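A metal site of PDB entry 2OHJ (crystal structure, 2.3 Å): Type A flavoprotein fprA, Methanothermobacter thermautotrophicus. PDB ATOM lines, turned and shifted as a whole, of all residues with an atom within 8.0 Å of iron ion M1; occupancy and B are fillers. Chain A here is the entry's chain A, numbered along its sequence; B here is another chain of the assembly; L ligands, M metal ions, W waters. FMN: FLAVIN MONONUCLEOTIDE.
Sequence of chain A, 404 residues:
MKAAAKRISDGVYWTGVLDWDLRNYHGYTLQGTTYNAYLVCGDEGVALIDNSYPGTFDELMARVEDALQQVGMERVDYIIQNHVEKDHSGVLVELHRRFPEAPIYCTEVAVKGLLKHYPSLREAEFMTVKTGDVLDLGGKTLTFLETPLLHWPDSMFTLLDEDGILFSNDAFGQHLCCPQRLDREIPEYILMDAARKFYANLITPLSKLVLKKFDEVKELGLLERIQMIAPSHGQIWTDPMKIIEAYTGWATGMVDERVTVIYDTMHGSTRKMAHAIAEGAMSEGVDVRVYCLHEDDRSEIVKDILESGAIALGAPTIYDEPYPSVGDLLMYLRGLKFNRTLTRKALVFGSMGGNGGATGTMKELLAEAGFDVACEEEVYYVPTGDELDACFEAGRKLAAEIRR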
ATOM      1  N   TYR A  25      -3.862 -29.393  27.743  1.00  0.00           N
ATOM      2  CA  TYR A  25      -3.591 -29.159  26.319  1.00  0.00           C
ATOM      3  C   TYR A  25      -2.372 -28.253  26.111  1.00  0.00           C
ATOM      4  O   TYR A  25      -2.001 -27.495  27.002  1.00  0.00           O
ATOM      5  CB  TYR A  25      -4.881 -28.697  25.577  1.00  0.00           C
ATOM      6  CG  TYR A  25      -5.152 -27.216  25.511  1.00  0.00           C
ATOM      7  CD1 TYR A  25      -5.727 -26.658  24.368  1.00  0.00           C
ATOM      8  CD2 TYR A  25      -4.855 -26.358  26.579  1.00  0.00           C
ATOM      9  CE1 TYR A  25      -5.992 -25.303  24.271  1.00  0.00           C
ATOM     10  CE2 TYR A  25      -5.110 -24.985  26.508  1.00  0.00           C
ATOM     11  CZ  TYR A  25      -5.684 -24.466  25.341  1.00  0.00           C
ATOM     12  OH  TYR A  25      -5.951 -23.099  25.237  1.00  0.00           O
ATOM     13  N   HIS A  26      -1.729 -28.357  24.944  1.00  0.00           N
ATOM     14  CA  HIS A  26      -0.499 -27.598  24.671  1.00  0.00           C
ATOM     15  C   HIS A  26       0.667 -27.897  25.640  1.00  0.00           C
ATOM     16  O   HIS A  26       1.529 -27.031  25.849  1.00  0.00           O
ATOM     17  CB  HIS A  26      -0.750 -26.079  24.715  1.00  0.00           C
ATOM     18  CG  HIS A  26      -1.732 -25.585  23.716  1.00  0.00           C
ATOM     19  ND1 HIS A  26      -2.452 -24.421  23.901  1.00  0.00           N
ATOM     20  CD2 HIS A  26      -2.135 -26.075  22.515  1.00  0.00           C
ATOM     21  CE1 HIS A  26      -3.235 -24.218  22.865  1.00  0.00           C
ATOM     22  NE2 HIS A  26      -3.064 -25.213  22.009  1.00  0.00           N
ATOM     23  N   TYR A  35     -12.223 -18.595  25.909  1.00  0.00           N
ATOM     24  CA  TYR A  35     -11.790 -17.980  24.671  1.00  0.00           C
ATOM     25  C   TYR A  35     -12.513 -16.651  24.574  1.00  0.00           C
ATOM     26  O   TYR A  35     -13.699 -16.594  24.254  1.00  0.00           O
ATOM     27  CB  TYR A  35     -12.088 -18.893  23.484  1.00  0.00           C
ATOM     28  CG  TYR A  35     -11.712 -20.308  23.805  1.00  0.00           C
ATOM     29  CD1 TYR A  35     -10.378 -20.641  24.036  1.00  0.00           C
ATOM     30  CD2 TYR A  35     -12.662 -21.287  23.951  1.00  0.00           C
ATOM     31  CE1 TYR A  35     -10.005 -21.939  24.371  1.00  0.00           C
ATOM     32  CE2 TYR A  35     -12.301 -22.593  24.277  1.00  0.00           C
ATOM     33  CZ  TYR A  35     -10.973 -22.902  24.494  1.00  0.00           C
ATOM     34  OH  TYR A  35     -10.602 -24.189  24.822  1.00  0.00           O
ATOM     35  N   TYR A  53     -12.651 -21.692  19.851  1.00  0.00           N
ATOM     36  CA  TYR A  53     -12.379 -23.082  19.458  1.00  0.00           C
ATOM     37  C   TYR A  53     -13.455 -23.648  18.512  1.00  0.00           C
ATOM     38  O   TYR A  53     -14.622 -23.265  18.599  1.00  0.00           O
ATOM     39  CB  TYR A  53     -12.230 -23.955  20.725  1.00  0.00           C
ATOM     40  CG  TYR A  53     -11.608 -25.305  20.472  1.00  0.00           C
ATOM     41  CD1 TYR A  53     -10.222 -25.463  20.447  1.00  0.00           C
ATOM     42  CD2 TYR A  53     -12.412 -26.443  20.265  1.00  0.00           C
ATOM     43  CE1 TYR A  53      -9.633 -26.693  20.225  1.00  0.00           C
ATOM     44  CE2 TYR A  53     -11.821 -27.712  20.019  1.00  0.00           C
ATOM     45  CZ  TYR A  53     -10.431 -27.824  20.015  1.00  0.00           C
ATOM     46  OH  TYR A  53      -9.809 -29.033  19.773  1.00  0.00           O
ATOM     47  N   VAL A  84      -3.780 -16.785  14.725  1.00  0.00           N
ATOM     48  CA  VAL A  84      -4.376 -17.884  13.942  1.00  0.00           C
ATOM     49  C   VAL A  84      -4.735 -19.130  14.764  1.00  0.00           C
ATOM     50  O   VAL A  84      -5.573 -19.926  14.344  1.00  0.00           O
ATOM     51  CB  VAL A  84      -3.512 -18.272  12.701  1.00  0.00           C
ATOM     52  CG1 VAL A  84      -3.158 -17.040  11.899  1.00  0.00           C
ATOM     53  CG2 VAL A  84      -2.259 -19.054  13.077  1.00  0.00           C
ATOM     54  N   GLU A  85      -4.074 -19.309  15.909  1.00  0.00           N
ATOM     55  CA  GLU A  85      -4.298 -20.449  16.805  1.00  0.00           C
ATOM     56  C   GLU A  85      -5.773 -20.857  16.853  1.00  0.00           C
ATOM     57  O   GLU A  85      -6.651 -20.002  16.985  1.00  0.00           O
ATOM     58  CB  GLU A  85      -3.720 -20.115  18.189  1.00  0.00           C
ATOM     59  CG  GLU A  85      -4.406 -20.728  19.392  1.00  0.00           C
ATOM     60  CD  GLU A  85      -4.069 -22.188  19.582  1.00  0.00           C
ATOM     61  OE1 GLU A  85      -5.010 -22.978  19.830  1.00  0.00           O
ATOM     62  OE2 GLU A  85      -2.877 -22.554  19.488  1.00  0.00           O
ATOM     63  N   LYS A  86      -6.051 -22.163  16.744  1.00  0.00           N
ATOM     64  CA  LYS A  86      -7.449 -22.617  16.539  1.00  0.00           C
ATOM     65  C   LYS A  86      -8.380 -22.315  17.716  1.00  0.00           C
ATOM     66  O   LYS A  86      -9.589 -22.159  17.510  1.00  0.00           O
ATOM     67  CB  LYS A  86      -7.543 -24.087  16.096  1.00  0.00           C
ATOM     68  CG  LYS A  86      -7.291 -25.129  17.173  1.00  0.00           C
ATOM     69  CD  LYS A  86      -7.075 -26.520  16.575  1.00  0.00           C
ATOM     70  CE  LYS A  86      -8.374 -27.262  16.317  1.00  0.00           C
ATOM     71  NZ  LYS A  86      -8.113 -28.722  16.242  1.00  0.00           N
ATOM     72  N   ASP A  87      -7.812 -22.229  18.928  1.00  0.00           N
ATOM     73  CA  ASP A  87      -8.500 -21.643  20.102  1.00  0.00           C
ATOM     74  C   ASP A  87      -9.205 -20.316  19.776  1.00  0.00           C
ATOM     75  O   ASP A  87     -10.202 -19.977  20.411  1.00  0.00           O
ATOM     76  CB  ASP A  87      -7.487 -21.334  21.199  1.00  0.00           C
ATOM     77  CG  ASP A  87      -7.068 -22.530  21.992  1.00  0.00           C
ATOM     78  OD1 ASP A  87      -6.317 -22.308  22.964  1.00  0.00           O
ATOM     79  OD2 ASP A  87      -7.465 -23.672  21.668  1.00  0.00           O
ATOM     80  N   HIS A  88      -8.663 -19.580  18.796  1.00  0.00           N
ATOM     81  CA  HIS A  88      -9.031 -18.178  18.577  1.00  0.00           C
ATOM     82  C   HIS A  88      -9.560 -17.892  17.190  1.00  0.00           C
ATOM     83  O   HIS A  88     -10.143 -16.837  16.968  1.00  0.00           O
ATOM     84  CB  HIS A  88      -7.840 -17.267  18.874  1.00  0.00           C
ATOM     85  CG  HIS A  88      -7.275 -17.484  20.238  1.00  0.00           C
ATOM     86  ND1 HIS A  88      -7.986 -17.227  21.389  1.00  0.00           N
ATOM     87  CD2 HIS A  88      -6.077 -17.971  20.633  1.00  0.00           C
ATOM     88  CE1 HIS A  88      -7.245 -17.541  22.436  1.00  0.00           C
ATOM     89  NE2 HIS A  88      -6.088 -17.993  22.016  1.00  0.00           N
ATOM     90  N   HIS A 117      -5.012 -23.518   7.588  1.00  0.00           N
ATOM     91  CA  HIS A 117      -6.036 -24.121   8.438  1.00  0.00           C
ATOM     92  C   HIS A 117      -7.395 -24.220   7.708  1.00  0.00           C
ATOM     93  O   HIS A 117      -8.082 -25.244   7.788  1.00  0.00           O
ATOM     94  CB  HIS A 117      -6.245 -23.312   9.721  1.00  0.00           C
ATOM     95  CG  HIS A 117      -5.177 -23.495  10.749  1.00  0.00           C
ATOM     96  ND1 HIS A 117      -4.031 -22.731  10.776  1.00  0.00           N
ATOM     97  CD2 HIS A 117      -5.108 -24.321  11.816  1.00  0.00           C
ATOM     98  CE1 HIS A 117      -3.295 -23.086  11.812  1.00  0.00           C
ATOM     99  NE2 HIS A 117      -3.922 -24.049  12.458  1.00  0.00           N
ATOM    100  N   ASP A 170      -2.839 -13.490  23.364  1.00  0.00           N
ATOM    101  CA  ASP A 170      -2.463 -14.339  24.510  1.00  0.00           C
ATOM    102  C   ASP A 170      -1.528 -13.692  25.540  1.00  0.00           C
ATOM    103  O   ASP A 170      -1.392 -14.189  26.670  1.00  0.00           O
ATOM    104  CB  ASP A 170      -1.955 -15.713  24.022  1.00  0.00           C
ATOM    105  CG  ASP A 170      -3.085 -16.708  23.759  1.00  0.00           C
ATOM    106  OD1 ASP A 170      -4.249 -16.293  23.607  1.00  0.00           O
ATOM    107  OD2 ASP A 170      -2.869 -17.927  23.724  1.00  0.00           O
ATOM    108  N   HIS A 233      -7.476 -15.275  26.956  1.00  0.00           N
ATOM    109  CA  HIS A 233      -7.850 -16.289  27.932  1.00  0.00           C
ATOM    110  C   HIS A 233      -7.928 -15.624  29.294  1.00  0.00           C
ATOM    111  O   HIS A 233      -7.069 -14.819  29.653  1.00  0.00           O
ATOM    112  CB  HIS A 233      -6.800 -17.394  28.037  1.00  0.00           C
ATOM    113  CG  HIS A 233      -6.520 -18.129  26.767  1.00  0.00           C
ATOM    114  ND1 HIS A 233      -7.305 -19.171  26.310  1.00  0.00           N
ATOM    115  CD2 HIS A 233      -5.492 -18.020  25.877  1.00  0.00           C
ATOM    116  CE1 HIS A 233      -6.795 -19.638  25.183  1.00  0.00           C
ATOM    117  NE2 HIS A 233      -5.693 -18.959  24.905  1.00  0.00           N
ATOM    118  N   MET B 266      -1.005 -31.983  19.090  1.00  0.00           N
ATOM    119  CA  MET B 266      -1.820 -31.050  19.884  1.00  0.00           C
ATOM    120  C   MET B 266      -3.146 -30.761  19.202  1.00  0.00           C
ATOM    121  O   MET B 266      -4.200 -30.837  19.836  1.00  0.00           O
ATOM    122  CB  MET B 266      -1.058 -29.749  20.165  1.00  0.00           C
ATOM    123  CG  MET B 266       0.115 -29.917  21.141  1.00  0.00           C
ATOM    124  SD  MET B 266       1.052 -28.387  21.395  1.00  0.00           S
ATOM    125  CE  MET B 266       1.733 -28.164  19.730  1.00  0.00           C
ATOM    126  N   HIS B 267      -3.089 -30.447  17.912  1.00  0.00           N
ATOM    127  CA  HIS B 267      -4.246 -30.025  17.130  1.00  0.00           C
ATOM    128  C   HIS B 267      -4.656 -31.069  16.084  1.00  0.00           C
ATOM    129  O   HIS B 267      -5.553 -30.815  15.283  1.00  0.00           O
ATOM    130  CB  HIS B 267      -3.942 -28.699  16.417  1.00  0.00           C
ATOM    131  CG  HIS B 267      -3.707 -27.540  17.337  1.00  0.00           C
ATOM    132  ND1 HIS B 267      -2.977 -26.430  16.969  1.00  0.00           N
ATOM    133  CD2 HIS B 267      -4.111 -27.312  18.616  1.00  0.00           C
ATOM    134  CE1 HIS B 267      -2.941 -25.569  17.965  1.00  0.00           C
ATOM    135  NE2 HIS B 267      -3.619 -26.076  18.980  1.00  0.00           N
HETATM  136  N1  FMN L   1       5.856 -23.970  15.621  1.00  0.00           N
HETATM  137  C2  FMN L   1       7.148 -23.701  15.210  1.00  0.00           C
HETATM  138  O2  FMN L   1       7.475 -23.848  14.037  1.00  0.00           O
HETATM  139  N3  FMN L   1       8.084 -23.291  16.110  1.00  0.00           N
HETATM  140  C4  FMN L   1       7.757 -23.115  17.429  1.00  0.00           C
HETATM  141  O4  FMN L   1       8.613 -22.664  18.202  1.00  0.00           O
HETATM  142  C4A FMN L   1       6.454 -23.369  17.854  1.00  0.00           C
HETATM  143  N5  FMN L   1       6.097 -23.194  19.181  1.00  0.00           N
HETATM  144  C5A FMN L   1       4.826 -23.461  19.629  1.00  0.00           C
HETATM  145  C6  FMN L   1       4.547 -23.277  20.985  1.00  0.00           C
HETATM  146  C7  FMN L   1       3.272 -23.532  21.483  1.00  0.00           C
HETATM  147  C7M FMN L   1       3.115 -23.688  22.971  1.00  0.00           C
HETATM  148  C8  FMN L   1       2.265 -23.982  20.609  1.00  0.00           C
HETATM  149  C8M FMN L   1       0.903 -24.370  21.138  1.00  0.00           C
HETATM  150  C9  FMN L   1       2.556 -24.156  19.237  1.00  0.00           C
HETATM  151  C9A FMN L   1       3.846 -23.904  18.730  1.00  0.00           C
HETATM  152  N10 FMN L   1       4.188 -24.075  17.387  1.00  0.00           N
HETATM  153  C10 FMN L   1       5.488 -23.809  16.955  1.00  0.00           C
HETATM  154  C1' FMN L   1       3.133 -24.325  16.320  1.00  0.00           C
HETATM  155  C2' FMN L   1       2.779 -25.814  16.156  1.00  0.00           C
HETATM  156  O2' FMN L   1       3.914 -26.615  15.875  1.00  0.00           O
HETATM  157  C3' FMN L   1       1.738 -25.955  15.028  1.00  0.00           C
HETATM  158  O3' FMN L   1       0.493 -25.500  15.481  1.00  0.00           O
HETATM  159  C4' FMN L   1       1.600 -27.385  14.486  1.00  0.00           C
HETATM  160  O4' FMN L   1       0.848 -27.322  13.291  1.00  0.00           O
HETATM  161  C5' FMN L   1       0.973 -28.337  15.497  1.00  0.00           C
HETATM  162  O5' FMN L   1       0.838 -29.643  14.966  1.00  0.00           O
HETATM  163  P   FMN L   1      -0.211 -30.695  15.594  1.00  0.00           P
HETATM  164  O1P FMN L   1      -1.487 -30.566  14.826  1.00  0.00           O
HETATM  165  O2P FMN L   1       0.246 -32.119  15.373  1.00  0.00           O
HETATM  166  O3P FMN L   1      -0.330 -30.457  17.068  1.00  0.00           O
HETATM  167 FE    FE M   1      -4.170 -24.883  20.322  1.00  0.00          FE
HETATM  168 FE    FE M   2      -4.555 -18.639  23.188  1.00  0.00          FE
HETATM  169  O   HOH W   1      -5.891 -25.477  20.631  1.00  0.00           O
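O3P of the ligand lies within hydrogen-bond range of N of His 267 of chain B, at 2.9 Å. The backbone NH (N) of Met 266 of chain B is in hydrogen-bond range of an oxygen (O3P) of the ligand (2.6 Å).
Iron ion M1 is bound by water W1 (1.8 Å), a ring nitrogen (NE2) of His 267 of chain B (1.9 Å), a ring nitrogen (NE2) of His 26 (2.0 Å) and the side-chain carboxylate of Glu 85 (2.1 Å). Slightly farther from iron ion M1 lies OE2 of Glu 85 (2.8 Å).
Asp 87 touches iron ion M1 (OD2 to FE, 3.8 Å). Four residues have an atom within 4 Å of iron ion M1: His 26, Glu 85, Asp 87 and His 267 of chain B. The nearest printed residue that does not touch iron ion M1 is Tyr 25 (4.4 Å).
OE1 of Glu 85 lies close to N of Asp 87, at 3.0 Å. O of His 267 of chain B sits at hydrogen-bond distance from NZ of Lys 86, at 3.4 Å. N of Tyr 53 sits at hydrogen-bond distance from O of Asp 87 (3.0 Å). OD1 of Asp 87 lies within hydrogen-bond range of OH of Tyr 25 (2.4 Å).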
